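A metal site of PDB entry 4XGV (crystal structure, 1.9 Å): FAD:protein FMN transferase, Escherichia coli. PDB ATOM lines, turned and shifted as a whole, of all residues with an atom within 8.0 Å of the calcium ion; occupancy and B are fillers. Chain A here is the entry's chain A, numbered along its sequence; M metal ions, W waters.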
ATOM      1  N   MET A 102       5.604   2.925  14.409  1.00  0.00           N
ATOM      2  CA  MET A 102       4.456   2.132  13.964  1.00  0.00           C
ATOM      3  C   MET A 102       4.354   0.898  14.857  1.00  0.00           C
ATOM      4  O   MET A 102       5.098  -0.055  14.687  1.00  0.00           O
ATOM      5  CB  MET A 102       4.595   1.725  12.498  1.00  0.00           C
ATOM      6  CG  MET A 102       3.343   1.873  11.689  1.00  0.00           C
ATOM      7  SD  MET A 102       1.993   0.778  12.145  1.00  0.00           S
ATOM      8  CE  MET A 102       2.684  -0.815  11.737  1.00  0.00           C
ATOM      9  N   LEU A 164      -4.827  -4.044  14.664  1.00  0.00           N
ATOM     10  CA  LEU A 164      -4.385  -3.954  13.279  1.00  0.00           C
ATOM     11  C   LEU A 164      -5.152  -2.901  12.494  1.00  0.00           C
ATOM     12  O   LEU A 164      -5.100  -2.868  11.261  1.00  0.00           O
ATOM     13  CB  LEU A 164      -4.514  -5.329  12.607  1.00  0.00           C
ATOM     14  CG  LEU A 164      -3.636  -6.419  13.241  1.00  0.00           C
ATOM     15  CD1 LEU A 164      -3.922  -7.780  12.612  1.00  0.00           C
ATOM     16  CD2 LEU A 164      -2.142  -6.080  13.149  1.00  0.00           C
ATOM     17  N   SER A 165      -5.862  -2.019  13.203  1.00  0.00           N
ATOM     18  CA  SER A 165      -6.694  -1.030  12.520  1.00  0.00           C
ATOM     19  C   SER A 165      -5.872  -0.089  11.627  1.00  0.00           C
ATOM     20  O   SER A 165      -6.373   0.406  10.622  1.00  0.00           O
ATOM     21  CB  SER A 165      -7.504  -0.221  13.541  1.00  0.00           C
ATOM     22  OG  SER A 165      -6.655   0.496  14.419  1.00  0.00           O
ATOM     23  N   THR A 166      -4.607   0.156  11.975  1.00  0.00           N
ATOM     24  CA  THR A 166      -3.789   1.076  11.195  1.00  0.00           C
ATOM     25  C   THR A 166      -3.224   0.440   9.905  1.00  0.00           C
ATOM     26  O   THR A 166      -2.620   1.140   9.098  1.00  0.00           O
ATOM     27  CB  THR A 166      -2.603   1.638  12.001  1.00  0.00           C
ATOM     28  OG1 THR A 166      -1.739   0.579  12.414  1.00  0.00           O
ATOM     29  CG2 THR A 166      -3.080   2.413  13.223  1.00  0.00           C
ATOM     30  N   VAL A 167      -3.427  -0.860   9.725  1.00  0.00           N
ATOM     31  CA  VAL A 167      -2.994  -1.535   8.501  1.00  0.00           C
ATOM     32  C   VAL A 167      -4.072  -2.347   7.801  1.00  0.00           C
ATOM     33  O   VAL A 167      -3.837  -2.874   6.721  1.00  0.00           O
ATOM     34  CB  VAL A 167      -1.805  -2.487   8.754  1.00  0.00           C
ATOM     35  CG1 VAL A 167      -0.565  -1.699   9.081  1.00  0.00           C
ATOM     36  CG2 VAL A 167      -2.116  -3.506   9.859  1.00  0.00           C
ATOM     37  N   GLY A 168      -5.266  -2.443   8.399  1.00  0.00           N
ATOM     38  CA  GLY A 168      -6.306  -3.295   7.866  1.00  0.00           C
ATOM     39  C   GLY A 168      -6.876  -2.825   6.545  1.00  0.00           C
ATOM     40  O   GLY A 168      -7.219  -3.636   5.694  1.00  0.00           O
ATOM     41  N   GLU A 169      -6.965  -1.511   6.367  1.00  0.00           N
ATOM     42  CA  GLU A 169      -7.498  -0.962   5.120  1.00  0.00           C
ATOM     43  C   GLU A 169      -6.579  -1.290   3.956  1.00  0.00           C
ATOM     44  O   GLU A 169      -7.041  -1.655   2.874  1.00  0.00           O
ATOM     45  CB  GLU A 169      -7.702   0.547   5.231  1.00  0.00           C
ATOM     46  CG  GLU A 169      -8.787   0.913   6.260  1.00  0.00           C
ATOM     47  CD  GLU A 169      -8.946   2.419   6.451  1.00  0.00           C
ATOM     48  OE1 GLU A 169      -8.160   3.206   5.873  1.00  0.00           O
ATOM     49  OE2 GLU A 169      -9.868   2.797   7.187  1.00  0.00           O
ATOM     50  N   GLY A 170      -5.271  -1.183   4.188  1.00  0.00           N
ATOM     51  CA  GLY A 170      -4.294  -1.504   3.159  1.00  0.00           C
ATOM     52  C   GLY A 170      -4.364  -2.976   2.791  1.00  0.00           C
ATOM     53  O   GLY A 170      -4.418  -3.327   1.626  1.00  0.00           O
ATOM     54  N   ALA A 195      -7.156   3.634   1.828  1.00  0.00           N
ATOM     55  CA  ALA A 195      -6.191   2.860   1.036  1.00  0.00           C
ATOM     56  C   ALA A 195      -6.748   2.537  -0.344  1.00  0.00           C
ATOM     57  O   ALA A 195      -7.911   2.173  -0.473  1.00  0.00           O
ATOM     58  CB  ALA A 195      -5.820   1.577   1.762  1.00  0.00           C
ATOM     59  N   SER A 234      -1.838   5.159   0.480  1.00  0.00           N
ATOM     60  CA  SER A 234      -2.549   5.325   1.741  1.00  0.00           C
ATOM     61  C   SER A 234      -2.162   6.660   2.366  1.00  0.00           C
ATOM     62  O   SER A 234      -1.048   7.154   2.177  1.00  0.00           O
ATOM     63  CB  SER A 234      -2.233   4.178   2.703  1.00  0.00           C
ATOM     64  OG  SER A 234      -3.074   4.249   3.844  1.00  0.00           O
ATOM     65  N   THR A 235      -3.101   7.221   3.106  1.00  0.00           N
ATOM     66  CA  THR A 235      -2.878   8.470   3.827  1.00  0.00           C
ATOM     67  C   THR A 235      -3.234   8.274   5.307  1.00  0.00           C
ATOM     68  O   THR A 235      -4.195   7.579   5.627  1.00  0.00           O
ATOM     69  CB  THR A 235      -3.702   9.622   3.250  1.00  0.00           C
ATOM     70  OG1 THR A 235      -3.325   9.846   1.895  1.00  0.00           O
ATOM     71  CG2 THR A 235      -3.477  10.909   4.037  1.00  0.00           C
ATOM     72  N   SER A 236      -2.424   8.879   6.171  1.00  0.00           N
ATOM     73  CA  SER A 236      -2.661   8.900   7.611  1.00  0.00           C
ATOM     74  C   SER A 236      -2.495  10.335   8.089  1.00  0.00           C
ATOM     75  O   SER A 236      -1.636  11.078   7.601  1.00  0.00           O
ATOM     76  CB  SER A 236      -1.686   7.971   8.336  1.00  0.00           C
ATOM     77  OG  SER A 236      -1.790   8.095   9.745  1.00  0.00           O
ATOM     78  N   GLY A 237      -3.325  10.737   9.048  1.00  0.00           N
ATOM     79  CA  GLY A 237      -3.265  12.104   9.533  1.00  0.00           C
ATOM     80  C   GLY A 237      -3.554  12.289  11.011  1.00  0.00           C
ATOM     81  O   GLY A 237      -3.819  11.333  11.743  1.00  0.00           O
ATOM     82  N   VAL A 269       0.385  12.376   6.185  1.00  0.00           N
ATOM     83  CA  VAL A 269       1.386  11.637   5.435  1.00  0.00           C
ATOM     84  C   VAL A 269       0.690  10.727   4.427  1.00  0.00           C
ATOM     85  O   VAL A 269      -0.190   9.946   4.787  1.00  0.00           O
ATOM     86  CB  VAL A 269       2.295  10.761   6.343  1.00  0.00           C
ATOM     87  CG1 VAL A 269       3.248   9.925   5.500  1.00  0.00           C
ATOM     88  CG2 VAL A 269       3.074  11.607   7.330  1.00  0.00           C
ATOM     89  N   ALA A 276      -0.804  -1.585  -1.102  1.00  0.00           N
ATOM     90  CA  ALA A 276      -1.507  -0.694  -0.171  1.00  0.00           C
ATOM     91  C   ALA A 276      -1.224  -1.058   1.277  1.00  0.00           C
ATOM     92  O   ALA A 276      -1.207  -0.172   2.141  1.00  0.00           O
ATOM     93  CB  ALA A 276      -2.995  -0.728  -0.447  1.00  0.00           C
ATOM     94  N   LEU A 277      -0.995  -2.334   1.558  1.00  0.00           N
ATOM     95  CA  LEU A 277      -0.641  -2.741   2.922  1.00  0.00           C
ATOM     96  C   LEU A 277       0.658  -2.056   3.377  1.00  0.00           C
ATOM     97  O   LEU A 277       0.749  -1.528   4.481  1.00  0.00           O
ATOM     98  CB  LEU A 277      -0.510  -4.255   3.038  1.00  0.00           C
ATOM     99  CG  LEU A 277       0.090  -4.774   4.354  1.00  0.00           C
ATOM    100  CD1 LEU A 277      -0.737  -4.285   5.550  1.00  0.00           C
ATOM    101  CD2 LEU A 277       0.172  -6.284   4.331  1.00  0.00           C
ATOM    102  N   GLU A 278       1.675  -2.080   2.515  1.00  0.00           N
ATOM    103  CA  GLU A 278       2.923  -1.394   2.845  1.00  0.00           C
ATOM    104  C   GLU A 278       2.689   0.095   3.051  1.00  0.00           C
ATOM    105  O   GLU A 278       3.240   0.680   3.964  1.00  0.00           O
ATOM    106  CB  GLU A 278       3.947  -1.573   1.728  1.00  0.00           C
ATOM    107  CG  GLU A 278       4.521  -2.936   1.581  1.00  0.00           C
ATOM    108  CD  GLU A 278       5.309  -3.051   0.284  1.00  0.00           C
ATOM    109  OE1 GLU A 278       6.533  -2.788   0.315  1.00  0.00           O
ATOM    110  OE2 GLU A 278       4.689  -3.349  -0.758  1.00  0.00           O
ATOM    111  N   ALA A 279       1.893   0.694   2.179  1.00  0.00           N
ATOM    112  CA  ALA A 279       1.617   2.124   2.256  1.00  0.00           C
ATOM    113  C   ALA A 279       0.929   2.463   3.577  1.00  0.00           C
ATOM    114  O   ALA A 279       1.259   3.464   4.230  1.00  0.00           O
ATOM    115  CB  ALA A 279       0.766   2.565   1.075  1.00  0.00           C
ATOM    116  N   ASP A 280      -0.011   1.614   3.958  1.00  0.00           N
ATOM    117  CA  ASP A 280      -0.798   1.810   5.153  1.00  0.00           C
ATOM    118  C   ASP A 280       0.042   1.575   6.425  1.00  0.00           C
ATOM    119  O   ASP A 280      -0.244   2.139   7.461  1.00  0.00           O
ATOM    120  CB  ASP A 280      -2.013   0.884   5.124  1.00  0.00           C
ATOM    121  CG  ASP A 280      -3.165   1.382   5.985  1.00  0.00           C
ATOM    122  OD1 ASP A 280      -3.121   2.539   6.447  1.00  0.00           O
ATOM    123  OD2 ASP A 280      -4.125   0.609   6.180  1.00  0.00           O
ATOM    124  N   ALA A 281       1.076   0.746   6.312  1.00  0.00           N
ATOM    125  CA  ALA A 281       1.999   0.525   7.425  1.00  0.00           C
ATOM    126  C   ALA A 281       2.909   1.738   7.586  1.00  0.00           C
ATOM    127  O   ALA A 281       3.031   2.301   8.673  1.00  0.00           O
ATOM    128  CB  ALA A 281       2.798  -0.731   7.204  1.00  0.00           C
ATOM    129  N   TRP A 282       3.549   2.158   6.495  1.00  0.00           N
ATOM    130  CA  TRP A 282       4.442   3.309   6.546  1.00  0.00           C
ATOM    131  C   TRP A 282       3.757   4.590   6.988  1.00  0.00           C
ATOM    132  O   TRP A 282       4.332   5.341   7.784  1.00  0.00           O
ATOM    133  CB  TRP A 282       5.093   3.567   5.184  1.00  0.00           C
ATOM    134  CG  TRP A 282       6.119   2.558   4.735  1.00  0.00           C
ATOM    135  CD1 TRP A 282       6.039   1.766   3.631  1.00  0.00           C
ATOM    136  CD2 TRP A 282       7.376   2.252   5.353  1.00  0.00           C
ATOM    137  NE1 TRP A 282       7.167   0.994   3.508  1.00  0.00           N
ATOM    138  CE2 TRP A 282       8.008   1.260   4.558  1.00  0.00           C
ATOM    139  CE3 TRP A 282       8.049   2.717   6.495  1.00  0.00           C
ATOM    140  CZ2 TRP A 282       9.248   0.728   4.865  1.00  0.00           C
ATOM    141  CZ3 TRP A 282       9.289   2.185   6.802  1.00  0.00           C
ATOM    142  CH2 TRP A 282       9.880   1.205   5.989  1.00  0.00           C
ATOM    143  N   ASP A 283       2.562   4.889   6.474  1.00  0.00           N
ATOM    144  CA  ASP A 283       2.017   6.242   6.624  1.00  0.00           C
ATOM    145  C   ASP A 283       1.777   6.562   8.100  1.00  0.00           C
ATOM    146  O   ASP A 283       2.043   7.667   8.566  1.00  0.00           O
ATOM    147  CB  ASP A 283       0.743   6.460   5.767  1.00  0.00           C
ATOM    148  CG  ASP A 283      -0.451   5.586   6.168  1.00  0.00           C
ATOM    149  OD1 ASP A 283      -0.438   4.871   7.196  1.00  0.00           O
ATOM    150  OD2 ASP A 283      -1.451   5.624   5.408  1.00  0.00           O
ATOM    151  N   THR A 284       1.331   5.554   8.844  1.00  0.00           N
ATOM    152  CA  THR A 284       1.093   5.698  10.279  1.00  0.00           C
ATOM    153  C   THR A 284       2.409   5.915  11.060  1.00  0.00           C
ATOM    154  O   THR A 284       2.499   6.804  11.921  1.00  0.00           O
ATOM    155  CB  THR A 284       0.358   4.466  10.799  1.00  0.00           C
ATOM    156  OG1 THR A 284      -0.961   4.442  10.238  1.00  0.00           O
ATOM    157  CG2 THR A 284       0.257   4.477  12.325  1.00  0.00           C
ATOM    158  N   GLY A 285       3.408   5.100  10.761  1.00  0.00           N
ATOM    159  CA  GLY A 285       4.715   5.243  11.388  1.00  0.00           C
ATOM    160  C   GLY A 285       5.364   6.586  11.123  1.00  0.00           C
ATOM    161  O   GLY A 285       5.921   7.211  12.038  1.00  0.00           O
ATOM    162  N   MET A 287       3.935   9.385  10.212  1.00  0.00           N
ATOM    163  CA  MET A 287       3.110  10.345  10.917  1.00  0.00           C
ATOM    164  C   MET A 287       3.539  10.511  12.392  1.00  0.00           C
ATOM    165  O   MET A 287       3.702  11.630  12.873  1.00  0.00           O
ATOM    166  CB  MET A 287       1.646   9.907  10.835  1.00  0.00           C
ATOM    167  CG  MET A 287       0.673  10.915  11.307  1.00  0.00           C
ATOM    168  SD  MET A 287       0.666  12.418  10.311  1.00  0.00           S
ATOM    169  CE  MET A 287      -0.254  13.371  11.511  1.00  0.00           C
HETATM  170 CA    CA M   1      -2.003   3.350   8.342  1.00  0.00          CA
HETATM  171  O   HOH W   1      -3.492   5.165   7.395  1.00  0.00           O
HETATM  172  O   HOH W   2      -3.787   4.168   9.617  1.00  0.00           O
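The nearest printed residue that does not touch the calcium ion is Ala 281 (4.5 Å).
The side-chain carboxylate of Asp 280 lies close to the side-chain hydroxyl of Ser 234 (3.1 Å).
The side-chain carboxylate (OD2) of Asp 280 sits at hydrogen-bond distance from the backbone NH (N) of Gly 170, at 2.9 Å.
The side-chain sulfur (SD) of Met 102 sits at hydrogen-bond distance from the side-chain hydroxyl (OG1) of Thr 166, 3.7 Å away.
The backbone NH (N) of Ser 236 is in hydrogen-bond range of the side-chain carboxylate (OD2) of Asp 283 (3.5 Å).
The side-chain carboxylate (OD2) of Asp 283 lies within hydrogen-bond range of the side-chain hydroxyl (OG) of Ser 234 (2.6 Å).
OD2 of Asp 283 sits close to N of Thr 235, at 3.3 Å.
The calcium ion is bound by O of Asp 280 (2.3 Å), water W2 (2.3 Å), OD1 of Asp 280 (2.3 Å), O of Thr 166 (2.4 Å), OG1 of Thr 284 (2.4 Å), OD1 of Asp 283 (2.5 Å) and water W1 (2.5 Å).
The calcium ion has seven donor atoms within binding distance.
Water W1 lies within hydrogen-bond range of the side-chain carboxylate (OD2) of Asp 283 (2.9 Å) and the backbone carbonyl oxygen (O) of Thr 235 (3.1 Å).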
